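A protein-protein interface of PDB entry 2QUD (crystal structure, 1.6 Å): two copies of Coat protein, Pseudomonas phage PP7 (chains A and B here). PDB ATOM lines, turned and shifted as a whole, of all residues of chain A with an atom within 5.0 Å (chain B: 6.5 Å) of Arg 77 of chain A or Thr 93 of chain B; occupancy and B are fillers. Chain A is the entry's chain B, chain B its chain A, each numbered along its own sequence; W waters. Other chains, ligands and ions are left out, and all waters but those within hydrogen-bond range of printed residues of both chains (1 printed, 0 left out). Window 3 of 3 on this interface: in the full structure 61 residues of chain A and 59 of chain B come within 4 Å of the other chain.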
ATOM      1  N   ASP A  67     -11.426  11.559  -0.365  1.00  0.00           N
ATOM      2  CA  ASP A  67     -10.373  10.975   0.433  1.00  0.00           C
ATOM      3  C   ASP A  67     -11.052  10.181   1.546  1.00  0.00           C
ATOM      4  O   ASP A  67     -11.769  10.753   2.380  1.00  0.00           O
ATOM      5  CB  ASP A  67      -9.499  12.088   1.004  1.00  0.00           C
ATOM      6  CG  ASP A  67      -8.118  11.621   1.347  1.00  0.00           C
ATOM      7  OD1 ASP A  67      -7.930  11.197   2.509  1.00  0.00           O
ATOM      8  OD2 ASP A  67      -7.226  11.685   0.465  1.00  0.00           O
ATOM      9  N   VAL A  68     -10.858   8.864   1.501  1.00  0.00           N
ATOM     10  CA  VAL A  68     -11.528   7.911   2.387  1.00  0.00           C
ATOM     11  C   VAL A  68     -10.555   7.496   3.477  1.00  0.00           C
ATOM     12  O   VAL A  68      -9.396   7.192   3.174  1.00  0.00           O
ATOM     13  CB  VAL A  68     -12.000   6.650   1.611  1.00  0.00           C
ATOM     14  CG1 VAL A  68     -12.623   5.624   2.564  1.00  0.00           C
ATOM     15  CG2 VAL A  68     -12.980   7.040   0.514  1.00  0.00           C
ATOM     16  N   VAL A  69     -11.037   7.497   4.723  1.00  0.00           N
ATOM     17  CA  VAL A  69     -10.223   7.179   5.899  1.00  0.00           C
ATOM     18  C   VAL A  69     -10.813   5.970   6.623  1.00  0.00           C
ATOM     19  O   VAL A  69     -10.381   4.840   6.400  1.00  0.00           O
ATOM     20  CB  VAL A  69     -10.125   8.401   6.859  1.00  0.00           C
ATOM     21  CG1 VAL A  69     -11.459   8.662   7.560  1.00  0.00           C
ATOM     22  CG2 VAL A  69      -8.998   8.202   7.872  1.00  0.00           C
ATOM     23  N   LYS A  75     -15.535   6.085   5.753  1.00  0.00           N
ATOM     24  CA  LYS A  75     -15.882   7.484   5.956  1.00  0.00           C
ATOM     25  C   LYS A  75     -15.087   8.356   4.974  1.00  0.00           C
ATOM     26  O   LYS A  75     -13.863   8.259   4.916  1.00  0.00           O
ATOM     27  CB  LYS A  75     -15.548   7.878   7.398  1.00  0.00           C
ATOM     28  CG  LYS A  75     -16.215   9.162   7.884  1.00  0.00           C
ATOM     29  CD  LYS A  75     -15.390   9.842   8.985  1.00  0.00           C
ATOM     30  CE  LYS A  75     -14.285  10.724   8.395  1.00  0.00           C
ATOM     31  NZ  LYS A  75     -13.217  11.082   9.375  1.00  0.00           N
ATOM     32  N   VAL A  76     -15.790   9.171   4.184  1.00  0.00           N
ATOM     33  CA  VAL A  76     -15.137  10.204   3.385  1.00  0.00           C
ATOM     34  C   VAL A  76     -14.785  11.344   4.345  1.00  0.00           C
ATOM     35  O   VAL A  76     -15.674  11.916   4.961  1.00  0.00           O
ATOM     36  CB  VAL A  76     -16.040  10.737   2.236  1.00  0.00           C
ATOM     37  CG1 VAL A  76     -15.389  11.974   1.544  1.00  0.00           C
ATOM     38  CG2 VAL A  76     -16.328   9.620   1.225  1.00  0.00           C
ATOM     39  N   ARG A  77     -13.496  11.642   4.507  1.00  0.00           N
ATOM     40  CA  ARG A  77     -13.125  12.793   5.340  1.00  0.00           C
ATOM     41  C   ARG A  77     -13.262  14.111   4.578  1.00  0.00           C
ATOM     42  O   ARG A  77     -13.637  15.116   5.154  1.00  0.00           O
ATOM     43  CB  ARG A  77     -11.744  12.647   6.007  1.00  0.00           C
ATOM     44  CG  ARG A  77     -10.570  12.233   5.150  1.00  0.00           C
ATOM     45  CD  ARG A  77      -9.293  12.359   5.982  1.00  0.00           C
ATOM     46  NE  ARG A  77      -8.106  11.838   5.301  1.00  0.00           N
ATOM     47  CZ  ARG A  77      -6.846  12.215   5.555  1.00  0.00           C
ATOM     48  NH1 ARG A  77      -5.851  11.677   4.850  1.00  0.00           N
ATOM     49  NH2 ARG A  77      -6.548  13.112   6.504  1.00  0.00           N
ATOM     50  N   TYR A  78     -12.957  14.112   3.280  1.00  0.00           N
ATOM     51  CA  TYR A  78     -13.130  15.314   2.473  1.00  0.00           C
ATOM     52  C   TYR A  78     -13.210  14.948   1.015  1.00  0.00           C
ATOM     53  O   TYR A  78     -12.803  13.843   0.643  1.00  0.00           O
ATOM     54  CB  TYR A  78     -11.995  16.333   2.712  1.00  0.00           C
ATOM     55  CG  TYR A  78     -10.578  15.841   2.432  1.00  0.00           C
ATOM     56  CD1 TYR A  78     -10.059  15.799   1.134  1.00  0.00           C
ATOM     57  CD2 TYR A  78      -9.738  15.457   3.472  1.00  0.00           C
ATOM     58  CE1 TYR A  78      -8.774  15.367   0.890  1.00  0.00           C
ATOM     59  CE2 TYR A  78      -8.432  15.019   3.228  1.00  0.00           C
ATOM     60  CZ  TYR A  78      -7.963  14.966   1.929  1.00  0.00           C
ATOM     61  OH  TYR A  78      -6.667  14.524   1.658  1.00  0.00           O
ATOM     62  N   THR A  79     -13.737  15.874   0.215  1.00  0.00           N
ATOM     63  CA  THR A  79     -13.799  15.717  -1.256  1.00  0.00           C
ATOM     64  C   THR A  79     -13.218  16.937  -1.922  1.00  0.00           C
ATOM     65  O   THR A  79     -13.515  18.074  -1.551  1.00  0.00           O
ATOM     66  CB  THR A  79     -15.251  15.547  -1.758  1.00  0.00           C
ATOM     67  OG1 THR A  79     -15.858  14.441  -1.064  1.00  0.00           O
ATOM     68  CG2 THR A  79     -15.297  15.295  -3.268  1.00  0.00           C
ATOM     69  N   VAL B  89      -9.112  21.330  -0.388  1.00  0.00           N
ATOM     70  CA  VAL B  89      -9.474  21.351   1.011  1.00  0.00           C
ATOM     71  C   VAL B  89      -8.249  21.653   1.866  1.00  0.00           C
ATOM     72  O   VAL B  89      -7.159  21.146   1.635  1.00  0.00           O
ATOM     73  CB  VAL B  89     -10.196  20.030   1.395  1.00  0.00           C
ATOM     74  CG1 VAL B  89     -10.464  19.986   2.885  1.00  0.00           C
ATOM     75  CG2 VAL B  89     -11.531  19.898   0.591  1.00  0.00           C
ATOM     76  N   ASN B  91      -7.278  20.939   4.922  1.00  0.00           N
ATOM     77  CA  ASN B  91      -6.678  19.831   5.671  1.00  0.00           C
ATOM     78  C   ASN B  91      -6.291  18.641   4.781  1.00  0.00           C
ATOM     79  O   ASN B  91      -6.024  17.551   5.261  1.00  0.00           O
ATOM     80  CB  ASN B  91      -7.587  19.401   6.837  1.00  0.00           C
ATOM     81  CG  ASN B  91      -8.796  18.579   6.399  1.00  0.00           C
ATOM     82  OD1 ASN B  91      -9.331  18.752   5.313  1.00  0.00           O
ATOM     83  ND2 ASN B  91      -9.252  17.691   7.283  1.00  0.00           N
ATOM     84  N   SER B  92      -6.236  18.851   3.471  1.00  0.00           N
ATOM     85  CA  SER B  92      -5.893  17.772   2.539  1.00  0.00           C
ATOM     86  C   SER B  92      -4.432  17.379   2.565  1.00  0.00           C
ATOM     87  O   SER B  92      -3.580  18.151   2.984  1.00  0.00           O
ATOM     88  CB  SER B  92      -6.296  18.155   1.113  1.00  0.00           C
ATOM     89  OG  SER B  92      -5.575  19.289   0.660  1.00  0.00           O
ATOM     90  N   THR B  93      -4.147  16.171   2.082  1.00  0.00           N
ATOM     91  CA  THR B  93      -2.779  15.768   1.850  1.00  0.00           C
ATOM     92  C   THR B  93      -2.254  16.303   0.524  1.00  0.00           C
ATOM     93  O   THR B  93      -3.011  16.454  -0.438  1.00  0.00           O
ATOM     94  CB  THR B  93      -2.639  14.231   1.820  1.00  0.00           C
ATOM     95  OG1 THR B  93      -3.374  13.715   0.710  1.00  0.00           O
ATOM     96  CG2 THR B  93      -3.162  13.580   3.143  1.00  0.00           C
ATOM     97  N   GLU B  94      -0.945  16.533   0.468  1.00  0.00           N
ATOM     98  CA  GLU B  94      -0.291  16.889  -0.790  1.00  0.00           C
ATOM     99  C   GLU B  94      -0.565  15.838  -1.868  1.00  0.00           C
ATOM    100  O   GLU B  94      -0.942  16.194  -2.977  1.00  0.00           O
ATOM    101  CB  GLU B  94       1.211  17.134  -0.607  1.00  0.00           C
ATOM    102  CG  GLU B  94       1.926  17.442  -1.918  1.00  0.00           C
ATOM    103  CD  GLU B  94       3.351  17.904  -1.752  1.00  0.00           C
ATOM    104  OE1 GLU B  94       4.122  17.741  -2.719  1.00  0.00           O
ATOM    105  OE2 GLU B  94       3.700  18.422  -0.684  1.00  0.00           O
ATOM    106  N   ALA B  95      -0.473  14.547  -1.504  1.00  0.00           N
ATOM    107  CA  ALA B  95      -0.696  13.472  -2.473  1.00  0.00           C
ATOM    108  C   ALA B  95      -2.083  13.552  -3.098  1.00  0.00           C
ATOM    109  O   ALA B  95      -2.241  13.318  -4.298  1.00  0.00           O
ATOM    110  CB  ALA B  95      -0.500  12.101  -1.815  1.00  0.00           C
ATOM    111  N   SER B  96      -3.082  13.941  -2.306  1.00  0.00           N
ATOM    112  CA  SER B  96      -4.462  14.045  -2.816  1.00  0.00           C
ATOM    113  C   SER B  96      -4.635  15.210  -3.807  1.00  0.00           C
ATOM    114  O   SER B  96      -5.346  15.092  -4.793  1.00  0.00           O
ATOM    115  CB  SER B  96      -5.513  14.183  -1.691  1.00  0.00           C
ATOM    116  OG  SER B  96      -5.411  15.403  -0.983  1.00  0.00           O
ATOM    117  N   ARG B  97      -3.993  16.332  -3.511  1.00  0.00           N
ATOM    118  CA  ARG B  97      -4.011  17.491  -4.408  1.00  0.00           C
ATOM    119  C   ARG B  97      -3.288  17.160  -5.709  1.00  0.00           C
ATOM    120  O   ARG B  97      -3.792  17.459  -6.785  1.00  0.00           O
ATOM    121  CB  ARG B  97      -3.381  18.709  -3.745  1.00  0.00           C
ATOM    122  CG  ARG B  97      -4.134  19.195  -2.509  1.00  0.00           C
ATOM    123  CD  ARG B  97      -3.619  20.482  -1.960  1.00  0.00           C
ATOM    124  NE  ARG B  97      -2.219  20.448  -1.534  1.00  0.00           N
ATOM    125  CZ  ARG B  97      -1.772  20.089  -0.335  1.00  0.00           C
ATOM    126  NH1 ARG B  97      -2.580  19.634   0.624  1.00  0.00           N
ATOM    127  NH2 ARG B  97      -0.472  20.164  -0.093  1.00  0.00           N
ATOM    128  N   LYS B  98      -2.107  16.535  -5.594  1.00  0.00           N
ATOM    129  CA  LYS B  98      -1.339  16.097  -6.766  1.00  0.00           C
ATOM    130  C   LYS B  98      -2.141  15.079  -7.581  1.00  0.00           C
ATOM    131  O   LYS B  98      -2.122  15.133  -8.805  1.00  0.00           O
ATOM    132  CB  LYS B  98       0.029  15.561  -6.338  1.00  0.00           C
ATOM    133  CG  LYS B  98       0.881  14.913  -7.385  1.00  0.00           C
ATOM    134  CD  LYS B  98       1.191  15.710  -8.623  1.00  0.00           C
ATOM    135  CE  LYS B  98       2.372  15.051  -9.340  1.00  0.00           C
ATOM    136  NZ  LYS B  98       2.565  15.527 -10.726  1.00  0.00           N
HETATM  137  O   HOH W   1      -4.302  11.220   0.728  1.00  0.00           O
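Among the printed residues, merely in contact across the chains: Thr 79 of chain A with Val 89 of chain B, Tyr 78 of chain A with Ser 92 of chain B, Arg 77 of chain A with Thr 93 of chain B, Asp 67 of chain A with Ser 96 of chain B, Tyr 78 of chain A with Asn 91 of chain B and Tyr 78 of chain A with Val 89 of chain B.
OH of Tyr 78 of chain A is in hydrogen-bond range of N of Thr 93 of chain B, 3.0 Å away.
The side-chain hydroxyl (OG) of Ser 96 of chain B is in hydrogen-bond range of the side-chain hydroxyl (OH) of Tyr 78 of chain A (3.1 Å).
No position is printed for both chains.
Of the 8 pairs that touch across the chains among the printed residues, none has its exchanged pair printed and touching as well.
Arg 77 of chain A touches just one residue of chain B: Thr 93.
Of the printed residues of chain A, Val 89 of chain B touches Tyr 78 (3.96 Å) and Thr 79 (3.4 Å).
Printed residues of chain A within 4 Å of Asn 91 of chain B: Tyr 78 (3.8 Å).
Thr 93 of chain B touches just these residues of chain A: Arg 77 and Tyr 78.
Glu 94 of chain B touches none of the printed residues of chain A.
The backbone carbonyl oxygen (O) of Thr 93 of chain B lies close to the guanidinium group (NH1) of Arg 97 of chain B (3.4 Å).
N of Asp 67 of chain A lies within hydrogen-bond range of O of Tyr 78 of chain A.
The side-chain carboxylate of Asp 67 of chain A is in salt-bridge range of the guanidinium group of Arg 77 of chain A (2.9 Å).
The backbone carbonyl oxygen (O) of Val 89 of chain B sits at hydrogen-bond distance from the side-chain hydroxyl (OG) of Ser 92 of chain B, at 2.6 Å.
The backbone carbonyl oxygen (O) of Thr 93 of chain B sits at hydrogen-bond distance from the side-chain hydroxyl (OG) of Ser 96 of chain B, 2.7 Å away.
NH1 of Arg 97 of chain B is in hydrogen-bond range of O of Ser 92 of chain B (3.0 Å).
Water W1 bridges the side-chain hydroxyl of Thr 93 of chain B (2.7 Å) and the side-chain carboxylate of Asp 67 of chain A (3.0 Å).
Hydrophobic or aromatic side chains of chain B that line the printed part of chain A: Val 89.
Printed residues of chain A that touch a printed residue of chain B: Asp 67, Arg 77, Tyr 78 and Thr 79.
Hydrophobic or aromatic side chains of chain A that line the printed part of chain B: Tyr 78.
Among the printed residues, 8 pairs touch across the chains.
Among the printed residues, no Asp or Glu carboxylate lies within 4 Å of a Lys or Arg side-chain nitrogen of the other chain.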
